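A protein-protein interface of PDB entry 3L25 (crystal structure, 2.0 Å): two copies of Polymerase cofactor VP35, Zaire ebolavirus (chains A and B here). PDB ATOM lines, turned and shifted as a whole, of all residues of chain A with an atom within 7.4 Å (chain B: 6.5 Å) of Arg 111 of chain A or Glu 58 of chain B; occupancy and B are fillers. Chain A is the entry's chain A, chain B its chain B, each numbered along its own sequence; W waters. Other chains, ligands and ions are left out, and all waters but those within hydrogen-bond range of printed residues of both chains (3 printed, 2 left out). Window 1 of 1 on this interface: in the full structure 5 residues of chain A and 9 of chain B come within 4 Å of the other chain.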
ATOM      1  N   THR A  70     -18.598  21.010 -20.668  1.00  0.00           N
ATOM      2  CA  THR A  70     -19.266  21.851 -21.674  1.00  0.00           C
ATOM      3  C   THR A  70     -20.527  22.480 -21.087  1.00  0.00           C
ATOM      4  O   THR A  70     -21.000  23.504 -21.568  1.00  0.00           O
ATOM      5  CB  THR A  70     -19.630  21.072 -22.953  1.00  0.00           C
ATOM      6  OG1 THR A  70     -20.607  20.069 -22.653  1.00  0.00           O
ATOM      7  CG2 THR A  70     -18.400  20.427 -23.579  1.00  0.00           C
ATOM      8  N   LYS A  71     -21.068  21.861 -20.038  1.00  0.00           N
ATOM      9  CA  LYS A  71     -22.274  22.395 -19.390  1.00  0.00           C
ATOM     10  C   LYS A  71     -21.976  23.352 -18.237  1.00  0.00           C
ATOM     11  O   LYS A  71     -22.810  24.200 -17.906  1.00  0.00           O
ATOM     12  CB  LYS A  71     -23.189  21.257 -18.932  1.00  0.00           C
ATOM     13  CG  LYS A  71     -23.747  20.440 -20.115  1.00  0.00           C
ATOM     14  CD  LYS A  71     -24.659  19.328 -19.667  1.00  0.00           C
ATOM     15  CE  LYS A  71     -25.168  18.534 -20.860  1.00  0.00           C
ATOM     16  NZ  LYS A  71     -26.477  17.876 -20.561  1.00  0.00           N
ATOM     17  N   PHE A  76     -18.053  27.716 -22.539  1.00  0.00           N
ATOM     18  CA  PHE A  76     -18.818  26.777 -23.371  1.00  0.00           C
ATOM     19  C   PHE A  76     -20.320  27.017 -23.348  1.00  0.00           C
ATOM     20  O   PHE A  76     -21.038  26.513 -24.207  1.00  0.00           O
ATOM     21  CB  PHE A  76     -18.512  25.331 -22.983  1.00  0.00           C
ATOM     22  CG  PHE A  76     -17.050  24.999 -23.043  1.00  0.00           C
ATOM     23  CD1 PHE A  76     -16.375  24.979 -24.270  1.00  0.00           C
ATOM     24  CD2 PHE A  76     -16.336  24.741 -21.877  1.00  0.00           C
ATOM     25  CE1 PHE A  76     -15.004  24.696 -24.313  1.00  0.00           C
ATOM     26  CE2 PHE A  76     -14.972  24.463 -21.918  1.00  0.00           C
ATOM     27  CZ  PHE A  76     -14.308  24.447 -23.130  1.00  0.00           C
ATOM     28  N   ASP A  78     -23.721  28.351 -24.047  1.00  0.00           N
ATOM     29  CA  ASP A  78     -24.368  29.019 -25.179  1.00  0.00           C
ATOM     30  C   ASP A  78     -23.372  29.352 -26.300  1.00  0.00           C
ATOM     31  O   ASP A  78     -23.632  30.223 -27.126  1.00  0.00           O
ATOM     32  CB  ASP A  78     -25.143  30.272 -24.704  1.00  0.00           C
ATOM     33  CG  ASP A  78     -26.537  30.373 -25.315  1.00  0.00           C
ATOM     34  OD1 ASP A  78     -27.113  29.317 -25.667  1.00  0.00           O
ATOM     35  OD2 ASP A  78     -27.073  31.507 -25.437  1.00  0.00           O
ATOM     36  N   ALA A  79     -22.243  28.645 -26.321  1.00  0.00           N
ATOM     37  CA  ALA A  79     -21.195  28.843 -27.331  1.00  0.00           C
ATOM     38  C   ALA A  79     -21.422  27.986 -28.580  1.00  0.00           C
ATOM     39  O   ALA A  79     -21.827  26.832 -28.479  1.00  0.00           O
ATOM     40  CB  ALA A  79     -19.820  28.530 -26.739  1.00  0.00           C
ATOM     41  N   ARG A 101     -23.577  15.232 -39.145  1.00  0.00           N
ATOM     42  CA  ARG A 101     -24.915  15.667 -39.566  1.00  0.00           C
ATOM     43  C   ARG A 101     -24.863  17.023 -40.251  1.00  0.00           C
ATOM     44  O   ARG A 101     -23.919  17.799 -40.039  1.00  0.00           O
ATOM     45  CB  ARG A 101     -25.842  15.909 -38.374  1.00  0.00           C
ATOM     46  CG  ARG A 101     -25.758  15.013 -37.225  1.00  0.00           C
ATOM     47  CD  ARG A 101     -26.870  15.419 -36.292  1.00  0.00           C
ATOM     48  NE  ARG A 101     -27.201  14.327 -35.402  1.00  0.00           N
ATOM     49  CZ  ARG A 101     -28.156  14.371 -34.487  1.00  0.00           C
ATOM     50  NH1 ARG A 101     -28.914  15.466 -34.331  1.00  0.00           N
ATOM     51  NH2 ARG A 101     -28.352  13.304 -33.738  1.00  0.00           N
ATOM     52  N   PRO A 102     -25.924  17.357 -41.008  1.00  0.00           N
ATOM     53  CA  PRO A 102     -26.026  18.728 -41.514  1.00  0.00           C
ATOM     54  C   PRO A 102     -26.097  19.687 -40.331  1.00  0.00           C
ATOM     55  O   PRO A 102     -26.681  19.364 -39.292  1.00  0.00           O
ATOM     56  CB  PRO A 102     -27.360  18.730 -42.273  1.00  0.00           C
ATOM     57  CG  PRO A 102     -27.644  17.307 -42.571  1.00  0.00           C
ATOM     58  CD  PRO A 102     -27.073  16.530 -41.422  1.00  0.00           C
ATOM     59  N   VAL A 103     -25.506  20.857 -40.483  1.00  0.00           N
ATOM     60  CA  VAL A 103     -25.410  21.807 -39.377  1.00  0.00           C
ATOM     61  C   VAL A 103     -26.740  22.587 -39.269  1.00  0.00           C
ATOM     62  O   VAL A 103     -27.233  23.098 -40.281  1.00  0.00           O
ATOM     63  CB  VAL A 103     -24.216  22.773 -39.618  1.00  0.00           C
ATOM     64  CG1 VAL A 103     -24.051  23.778 -38.481  1.00  0.00           C
ATOM     65  CG2 VAL A 103     -22.918  21.964 -39.842  1.00  0.00           C
ATOM     66  N   PRO A 104     -27.317  22.689 -38.048  1.00  0.00           N
ATOM     67  CA  PRO A 104     -28.518  23.500 -37.905  1.00  0.00           C
ATOM     68  C   PRO A 104     -28.175  24.996 -37.843  1.00  0.00           C
ATOM     69  O   PRO A 104     -26.998  25.349 -37.783  1.00  0.00           O
ATOM     70  CB  PRO A 104     -29.092  23.028 -36.567  1.00  0.00           C
ATOM     71  CG  PRO A 104     -27.912  22.601 -35.780  1.00  0.00           C
ATOM     72  CD  PRO A 104     -26.898  22.099 -36.759  1.00  0.00           C
ATOM     73  N   PRO A 105     -29.189  25.878 -37.871  1.00  0.00           N
ATOM     74  CA  PRO A 105     -28.892  27.318 -37.816  1.00  0.00           C
ATOM     75  C   PRO A 105     -28.140  27.822 -36.561  1.00  0.00           C
ATOM     76  O   PRO A 105     -27.325  28.737 -36.691  1.00  0.00           O
ATOM     77  CB  PRO A 105     -30.275  27.968 -37.938  1.00  0.00           C
ATOM     78  CG  PRO A 105     -31.115  26.925 -38.622  1.00  0.00           C
ATOM     79  CD  PRO A 105     -30.636  25.635 -38.011  1.00  0.00           C
ATOM     80  N   SER A 106     -28.387  27.249 -35.380  1.00  0.00           N
ATOM     81  CA  SER A 106     -27.684  27.710 -34.168  1.00  0.00           C
ATOM     82  C   SER A 106     -27.137  26.599 -33.269  1.00  0.00           C
ATOM     83  O   SER A 106     -27.617  26.427 -32.153  1.00  0.00           O
ATOM     84  CB  SER A 106     -28.569  28.659 -33.343  1.00  0.00           C
ATOM     85  OG  SER A 106     -28.837  29.853 -34.058  1.00  0.00           O
ATOM     86  N   PRO A 107     -26.114  25.857 -33.738  1.00  0.00           N
ATOM     87  CA  PRO A 107     -25.593  24.762 -32.904  1.00  0.00           C
ATOM     88  C   PRO A 107     -24.880  25.292 -31.659  1.00  0.00           C
ATOM     89  O   PRO A 107     -24.275  26.358 -31.700  1.00  0.00           O
ATOM     90  CB  PRO A 107     -24.602  24.032 -33.826  1.00  0.00           C
ATOM     91  CG  PRO A 107     -24.224  25.053 -34.879  1.00  0.00           C
ATOM     92  CD  PRO A 107     -25.397  25.984 -35.023  1.00  0.00           C
ATOM     93  N   LYS A 108     -24.977  24.535 -30.569  1.00  0.00           N
ATOM     94  CA  LYS A 108     -24.396  24.888 -29.277  1.00  0.00           C
ATOM     95  C   LYS A 108     -23.526  23.749 -28.794  1.00  0.00           C
ATOM     96  O   LYS A 108     -23.944  22.578 -28.850  1.00  0.00           O
ATOM     97  CB  LYS A 108     -25.503  25.105 -28.243  1.00  0.00           C
ATOM     98  CG  LYS A 108     -26.512  26.164 -28.625  1.00  0.00           C
ATOM     99  CD  LYS A 108     -25.915  27.543 -28.603  1.00  0.00           C
ATOM    100  CE  LYS A 108     -26.989  28.578 -28.960  1.00  0.00           C
ATOM    101  NZ  LYS A 108     -26.394  29.738 -29.652  1.00  0.00           N
ATOM    102  N   ILE A 109     -22.333  24.089 -28.309  1.00  0.00           N
ATOM    103  CA  ILE A 109     -21.417  23.094 -27.737  1.00  0.00           C
ATOM    104  C   ILE A 109     -22.103  22.365 -26.578  1.00  0.00           C
ATOM    105  O   ILE A 109     -22.016  21.133 -26.477  1.00  0.00           O
ATOM    106  CB  ILE A 109     -20.056  23.712 -27.293  1.00  0.00           C
ATOM    107  CG1 ILE A 109     -19.234  24.164 -28.502  1.00  0.00           C
ATOM    108  CG2 ILE A 109     -19.224  22.705 -26.511  1.00  0.00           C
ATOM    109  CD1 ILE A 109     -18.030  25.065 -28.139  1.00  0.00           C
ATOM    110  N   ASP A 110     -22.822  23.098 -25.732  1.00  0.00           N
ATOM    111  CA  ASP A 110     -23.488  22.460 -24.590  1.00  0.00           C
ATOM    112  C   ASP A 110     -24.728  21.642 -24.950  1.00  0.00           C
ATOM    113  O   ASP A 110     -25.352  21.068 -24.068  1.00  0.00           O
ATOM    114  CB  ASP A 110     -23.738  23.422 -23.407  1.00  0.00           C
ATOM    115  CG  ASP A 110     -24.687  24.561 -23.741  1.00  0.00           C
ATOM    116  OD1 ASP A 110     -25.248  24.606 -24.863  1.00  0.00           O
ATOM    117  OD2 ASP A 110     -24.858  25.448 -22.871  1.00  0.00           O
ATOM    118  N   ARG A 111     -25.073  21.587 -26.237  1.00  0.00           N
ATOM    119  CA  ARG A 111     -26.075  20.626 -26.730  1.00  0.00           C
ATOM    120  C   ARG A 111     -25.431  19.503 -27.557  1.00  0.00           C
ATOM    121  O   ARG A 111     -26.119  18.707 -28.212  1.00  0.00           O
ATOM    122  CB  ARG A 111     -27.183  21.342 -27.502  1.00  0.00           C
ATOM    123  CG  ARG A 111     -28.051  22.238 -26.614  1.00  0.00           C
ATOM    124  CD  ARG A 111     -29.126  22.957 -27.422  1.00  0.00           C
ATOM    125  NE  ARG A 111     -30.150  22.045 -27.961  1.00  0.00           N
ATOM    126  CZ  ARG A 111     -31.190  21.581 -27.277  1.00  0.00           C
ATOM    127  NH1 ARG A 111     -31.357  21.887 -25.991  1.00  0.00           N
ATOM    128  NH2 ARG A 111     -32.062  20.780 -27.878  1.00  0.00           N
ATOM    129  N   GLY A 112     -24.103  19.435 -27.518  1.00  0.00           N
ATOM    130  CA  GLY A 112     -23.386  18.297 -28.074  1.00  0.00           C
ATOM    131  C   GLY A 112     -22.765  18.519 -29.440  1.00  0.00           C
ATOM    132  O   GLY A 112     -22.217  17.596 -30.009  1.00  0.00           O
ATOM    133  N   TRP A 113     -22.855  19.731 -29.973  1.00  0.00           N
ATOM    134  CA  TRP A 113     -22.198  20.073 -31.246  1.00  0.00           C
ATOM    135  C   TRP A 113     -20.736  20.405 -30.971  1.00  0.00           C
ATOM    136  O   TRP A 113     -20.423  21.473 -30.441  1.00  0.00           O
ATOM    137  CB  TRP A 113     -22.917  21.249 -31.911  1.00  0.00           C
ATOM    138  CG  TRP A 113     -24.295  20.886 -32.334  1.00  0.00           C
ATOM    139  CD1 TRP A 113     -25.452  21.135 -31.653  1.00  0.00           C
ATOM    140  CD2 TRP A 113     -24.674  20.179 -33.527  1.00  0.00           C
ATOM    141  NE1 TRP A 113     -26.527  20.634 -32.354  1.00  0.00           N
ATOM    142  CE2 TRP A 113     -26.078  20.050 -33.510  1.00  0.00           C
ATOM    143  CE3 TRP A 113     -23.957  19.645 -34.616  1.00  0.00           C
ATOM    144  CZ2 TRP A 113     -26.787  19.396 -34.526  1.00  0.00           C
ATOM    145  CZ3 TRP A 113     -24.670  18.995 -35.634  1.00  0.00           C
ATOM    146  CH2 TRP A 113     -26.069  18.887 -35.579  1.00  0.00           C
ATOM    147  N   VAL A 114     -19.857  19.462 -31.289  1.00  0.00           N
ATOM    148  CA  VAL A 114     -18.439  19.538 -30.957  1.00  0.00           C
ATOM    149  C   VAL A 114     -17.711  20.529 -31.856  1.00  0.00           C
ATOM    150  O   VAL A 114     -16.914  21.333 -31.384  1.00  0.00           O
ATOM    151  CB  VAL A 114     -17.751  18.159 -31.128  1.00  0.00           C
ATOM    152  CG1 VAL A 114     -16.239  18.277 -30.928  1.00  0.00           C
ATOM    153  CG2 VAL A 114     -18.360  17.121 -30.185  1.00  0.00           C
ATOM    154  N   LYS A 128     -21.760  15.715 -33.924  1.00  0.00           N
ATOM    155  CA  LYS A 128     -22.709  15.755 -32.806  1.00  0.00           C
ATOM    156  C   LYS A 128     -22.497  14.598 -31.833  1.00  0.00           C
ATOM    157  O   LYS A 128     -22.372  13.438 -32.253  1.00  0.00           O
ATOM    158  CB  LYS A 128     -24.147  15.739 -33.344  1.00  0.00           C
ATOM    159  CG  LYS A 128     -25.274  15.744 -32.299  1.00  0.00           C
ATOM    160  CD  LYS A 128     -25.507  17.122 -31.708  1.00  0.00           C
ATOM    161  CE  LYS A 128     -26.900  17.221 -31.112  1.00  0.00           C
ATOM    162  NZ  LYS A 128     -27.028  16.463 -29.843  1.00  0.00           N
ATOM    163  N   ILE A 129     -22.441  14.923 -30.540  1.00  0.00           N
ATOM    164  CA  ILE A 129     -22.577  13.913 -29.457  1.00  0.00           C
ATOM    165  C   ILE A 129     -24.022  13.956 -28.909  1.00  0.00           C
ATOM    166  O   ILE A 129     -24.633  15.038 -28.704  1.00  0.00           O
ATOM    167  CB  ILE A 129     -21.545  14.139 -28.312  1.00  0.00           C
ATOM    168  CG1 ILE A 129     -20.122  14.086 -28.882  1.00  0.00           C
ATOM    169  CG2 ILE A 129     -21.714  13.093 -27.218  1.00  0.00           C
ATOM    170  CD1 ILE A 129     -18.972  14.145 -27.837  1.00  0.00           C
ATOM    171  OXT ILE A 129     -24.658  12.926 -28.688  1.00  0.00           O
ATOM    172  N   ALA B  50     -40.778  21.967 -25.178  1.00  0.00           N
ATOM    173  CA  ALA B  50     -39.787  22.806 -25.869  1.00  0.00           C
ATOM    174  C   ALA B  50     -38.482  22.053 -26.199  1.00  0.00           C
ATOM    175  O   ALA B  50     -37.935  22.207 -27.294  1.00  0.00           O
ATOM    176  CB  ALA B  50     -39.498  24.095 -25.069  1.00  0.00           C
ATOM    177  N   GLU B  51     -37.999  21.238 -25.259  1.00  0.00           N
ATOM    178  CA  GLU B  51     -36.765  20.463 -25.449  1.00  0.00           C
ATOM    179  C   GLU B  51     -36.946  19.382 -26.521  1.00  0.00           C
ATOM    180  O   GLU B  51     -36.039  19.117 -27.323  1.00  0.00           O
ATOM    181  CB  GLU B  51     -36.318  19.811 -24.126  1.00  0.00           C
ATOM    182  CG  GLU B  51     -35.020  18.973 -24.224  1.00  0.00           C
ATOM    183  CD  GLU B  51     -33.888  19.704 -24.979  1.00  0.00           C
ATOM    184  OE1 GLU B  51     -33.600  20.884 -24.653  1.00  0.00           O
ATOM    185  OE2 GLU B  51     -33.291  19.092 -25.905  1.00  0.00           O
ATOM    186  N   GLN B  53     -39.046  19.443 -29.102  1.00  0.00           N
ATOM    187  CA  GLN B  53     -39.055  20.114 -30.397  1.00  0.00           C
ATOM    188  C   GLN B  53     -37.684  20.638 -30.824  1.00  0.00           C
ATOM    189  O   GLN B  53     -37.333  20.563 -31.998  1.00  0.00           O
ATOM    190  CB  GLN B  53     -40.085  21.251 -30.402  1.00  0.00           C
ATOM    191  CG  GLN B  53     -41.539  20.785 -30.124  1.00  0.00           C
ATOM    192  CD  GLN B  53     -42.074  19.722 -31.111  1.00  0.00           C
ATOM    193  OE1 GLN B  53     -41.444  19.410 -32.135  1.00  0.00           O
ATOM    194  NE2 GLN B  53     -43.254  19.175 -30.801  1.00  0.00           N
ATOM    195  N   ALA B  54     -36.931  21.187 -29.881  1.00  0.00           N
ATOM    196  CA  ALA B  54     -35.581  21.675 -30.157  1.00  0.00           C
ATOM    197  C   ALA B  54     -34.665  20.541 -30.596  1.00  0.00           C
ATOM    198  O   ALA B  54     -33.831  20.717 -31.488  1.00  0.00           O
ATOM    199  CB  ALA B  54     -35.000  22.390 -28.933  1.00  0.00           C
ATOM    200  N   SER B  55     -34.831  19.367 -29.987  1.00  0.00           N
ATOM    201  CA  SER B  55     -33.987  18.226 -30.326  1.00  0.00           C
ATOM    202  C   SER B  55     -34.342  17.672 -31.711  1.00  0.00           C
ATOM    203  O   SER B  55     -33.449  17.366 -32.511  1.00  0.00           O
ATOM    204  CB  SER B  55     -34.072  17.135 -29.247  1.00  0.00           C
ATOM    205  OG  SER B  55     -33.320  17.514 -28.094  1.00  0.00           O
ATOM    206  N   LEU B  56     -35.639  17.542 -31.992  1.00  0.00           N
ATOM    207  CA  LEU B  56     -36.095  17.143 -33.329  1.00  0.00           C
ATOM    208  C   LEU B  56     -35.599  18.114 -34.398  1.00  0.00           C
ATOM    209  O   LEU B  56     -35.144  17.691 -35.455  1.00  0.00           O
ATOM    210  CB  LEU B  56     -37.624  17.020 -33.386  1.00  0.00           C
ATOM    211  CG  LEU B  56     -38.278  15.941 -32.507  1.00  0.00           C
ATOM    212  CD1 LEU B  56     -39.791  15.979 -32.721  1.00  0.00           C
ATOM    213  CD2 LEU B  56     -37.729  14.564 -32.811  1.00  0.00           C
ATOM    214  N   ALA B  57     -35.659  19.410 -34.098  1.00  0.00           N
ATOM    215  CA  ALA B  57     -35.200  20.462 -35.018  1.00  0.00           C
ATOM    216  C   ALA B  57     -33.703  20.397 -35.350  1.00  0.00           C
ATOM    217  O   ALA B  57     -33.274  20.905 -36.384  1.00  0.00           O
ATOM    218  CB  ALA B  57     -35.546  21.841 -34.456  1.00  0.00           C
ATOM    219  N   GLU B  58     -32.894  19.804 -34.476  1.00  0.00           N
ATOM    220  CA  GLU B  58     -31.462  19.713 -34.787  1.00  0.00           C
ATOM    221  C   GLU B  58     -31.075  18.318 -35.310  1.00  0.00           C
ATOM    222  O   GLU B  58     -29.893  18.001 -35.475  1.00  0.00           O
ATOM    223  CB  GLU B  58     -30.573  20.244 -33.639  1.00  0.00           C
ATOM    224  CG  GLU B  58     -30.634  19.484 -32.331  1.00  0.00           C
ATOM    225  CD  GLU B  58     -29.955  20.240 -31.171  1.00  0.00           C
ATOM    226  OE1 GLU B  58     -29.076  21.094 -31.416  1.00  0.00           O
ATOM    227  OE2 GLU B  58     -30.299  19.968 -30.004  1.00  0.00           O
ATOM    228  N   GLY B  59     -32.096  17.508 -35.591  1.00  0.00           N
ATOM    229  CA  GLY B  59     -31.926  16.272 -36.338  1.00  0.00           C
ATOM    230  C   GLY B  59     -31.916  15.013 -35.505  1.00  0.00           C
ATOM    231  O   GLY B  59     -31.542  13.947 -36.005  1.00  0.00           O
ATOM    232  N   ASP B  60     -32.306  15.124 -34.231  1.00  0.00           N
ATOM    233  CA  ASP B  60     -32.365  13.964 -33.361  1.00  0.00           C
ATOM    234  C   ASP B  60     -33.569  13.109 -33.732  1.00  0.00           C
ATOM    235  O   ASP B  60     -34.625  13.640 -34.066  1.00  0.00           O
ATOM    236  CB  ASP B  60     -32.471  14.396 -31.899  1.00  0.00           C
ATOM    237  CG  ASP B  60     -31.141  14.905 -31.325  1.00  0.00           C
ATOM    238  OD1 ASP B  60     -30.056  14.723 -31.953  1.00  0.00           O
ATOM    239  OD2 ASP B  60     -31.185  15.477 -30.207  1.00  0.00           O
ATOM    240  N   GLN B  68     -32.862  12.997 -24.566  1.00  0.00           N
ATOM    241  CA  GLN B  68     -32.365  14.355 -24.320  1.00  0.00           C
ATOM    242  C   GLN B  68     -33.150  15.059 -23.215  1.00  0.00           C
ATOM    243  O   GLN B  68     -32.575  15.796 -22.420  1.00  0.00           O
ATOM    244  CB  GLN B  68     -32.429  15.233 -25.567  1.00  0.00           C
ATOM    245  CG  GLN B  68     -31.693  14.726 -26.806  1.00  0.00           C
ATOM    246  CD  GLN B  68     -30.205  14.640 -26.624  1.00  0.00           C
ATOM    247  OE1 GLN B  68     -29.706  14.549 -25.496  1.00  0.00           O
ATOM    248  NE2 GLN B  68     -29.468  14.658 -27.741  1.00  0.00           N
ATOM    249  N   ARG B  72     -31.588  16.819 -19.854  1.00  0.00           N
ATOM    250  CA  ARG B  72     -31.561  18.282 -19.901  1.00  0.00           C
ATOM    251  C   ARG B  72     -32.616  18.971 -19.050  1.00  0.00           C
ATOM    252  O   ARG B  72     -32.451  20.140 -18.701  1.00  0.00           O
ATOM    253  CB  ARG B  72     -31.663  18.774 -21.349  1.00  0.00           C
ATOM    254  CG  ARG B  72     -30.463  18.397 -22.202  1.00  0.00           C
ATOM    255  CD  ARG B  72     -30.683  18.757 -23.668  1.00  0.00           C
ATOM    256  NE  ARG B  72     -29.509  18.458 -24.475  1.00  0.00           N
ATOM    257  CZ  ARG B  72     -29.540  18.213 -25.785  1.00  0.00           C
ATOM    258  NH1 ARG B  72     -30.698  18.205 -26.436  1.00  0.00           N
ATOM    259  NH2 ARG B  72     -28.418  17.950 -26.443  1.00  0.00           N
HETATM  260  O   HOH W   1     -28.957  17.981 -38.520  1.00  0.00           O
HETATM  261  O   HOH W   2     -27.788  23.396 -30.508  1.00  0.00           O
HETATM  262  O   HOH W   3     -25.769  16.098 -26.652  1.00  0.00           O
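The guanidinium group (NH1) of Arg 101 of chain A lies within salt-bridge range of the side-chain carboxylate (OD1) of Asp 60 of chain B (2.7 Å). The guanidinium group of Arg 111 of chain A lies within salt-bridge range of the side-chain carboxylate of Glu 51 of chain B, 2.8 Å away. O of Arg 111 of chain A sits at hydrogen-bond distance from NH2 of Arg 72 of chain B. NH1 of Arg 101 of chain A is in hydrogen-bond range of O of Glu 58 of chain B. The side-chain carboxylate (OE1) of Glu 58 of chain B is in hydrogen-bond range of the indole nitrogen (NE1) of Trp 113 of chain A, 2.8 Å away. The guanidinium group (NH1) of Arg 101 of chain A lies close to the backbone carbonyl oxygen (O) of Gly 59 of chain B, at 3.5 Å. The guanidinium group (NH2) of Arg 111 of chain A is in salt-bridge range of the side-chain carboxylate (OE2) of Glu 58 of chain B.
Glu 58 of chain B touches just these residues of chain A: Arg 101, Arg 111 and Trp 113. No residue of chain A comes within 4 Å of Ala 57 of chain B. Of the printed residues of chain A, Gln 68 of chain B touches Lys 128 (3.7 Å). Printed residues of chain A within 4 Å of Ser 55 of chain B: Arg 111. Of the printed residues of chain B, Trp 113 of chain A touches Glu 58 (2.8 Å). Of the printed residues of chain B, Arg 101 of chain A touches Glu 58, Gly 59 and Asp 60. Of the printed residues of chain B, Lys 128 of chain A touches Gln 68 and Arg 72. The nearest residue of chain A that does not touch Glu 58 of chain B is Pro 104 of chain A (4.1 Å). The nearest printed residue of chain A that does not touch Gly 59 of chain B is Trp 113 of chain A (5.7 Å).
The side-chain hydroxyl (OG) of Ser 55 of chain B sits at hydrogen-bond distance from the guanidinium group (NH1) of Arg 72 of chain B. The backbone carbonyl oxygen of Arg 111 of chain A lies within hydrogen-bond range of the side-chain amino group of Lys 128 of chain A, 2.9 Å away. The side-chain hydroxyl (OG) of Ser 55 of chain B is in hydrogen-bond range of the side-chain carboxylate (OE2) of Glu 51 of chain B (2.7 Å). O of Lys 108 of chain A is in hydrogen-bond range of N of Trp 113 of chain A (3.2 Å). The guanidinium group of Arg 72 of chain B is in salt-bridge range of the side-chain carboxylate of Glu 58 of chain B (3.9997 Å). N of Asp 60 of chain B lies within hydrogen-bond range of O of Ser 55 of chain B (3.0 Å).
CB of Ala 54 of chain B touches NH2 of Arg 111 of chain A (3.5 Å). Arg 111 of chain A touches Ser 55 of chain B. NZ of Lys 128 of chain A touches NE2 of Gln 68 of chain B, at 3.7 Å. NZ of Lys 128 of chain A touches NH2 of Arg 72 of chain B (3.96 Å).
Water W3 lies within hydrogen-bond range of O of Ile 129 of chain A (2.6 Å), O of Arg 111 of chain A (3.1 Å), NH2 of Arg 72 of chain B (3.2 Å) and NZ of Lys 128 of chain A (3.4 Å). Water W1 bridges the backbone carbonyl oxygen (O) of Pro 102 of chain A (2.8 Å) and the backbone carbonyl oxygen (O) of Glu 58 of chain B (3.2 Å). Water W2 lies within hydrogen-bond range of OE1 of Glu 58 of chain B (2.8 Å), N of Lys 108 of chain A (3.0 Å) and O of Ser 106 of chain A (3.5 Å).
No position is printed for both chains. Of the 11 pairs that touch across the chains among the printed residues, none has its exchanged pair printed and touching as well.
Printed residues of chain A that touch a printed residue of chain B: Arg 101, Arg 111, Trp 113 and Lys 128. Hydrophobic or aromatic side chains of chain A within 4 Å of the printed part of chain B: Trp 113. Among the printed residues, 11 pairs touch across the chains. Among the printed residues, Asp or Glu carboxylates within 4 Å of a Lys or Arg side-chain nitrogen of the other chain: Arg 101 of chain A with Asp 60 of chain B, Arg 111 of chain A with Glu 51 of chain B and Arg 111 of chain A with Glu 58 of chain B.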
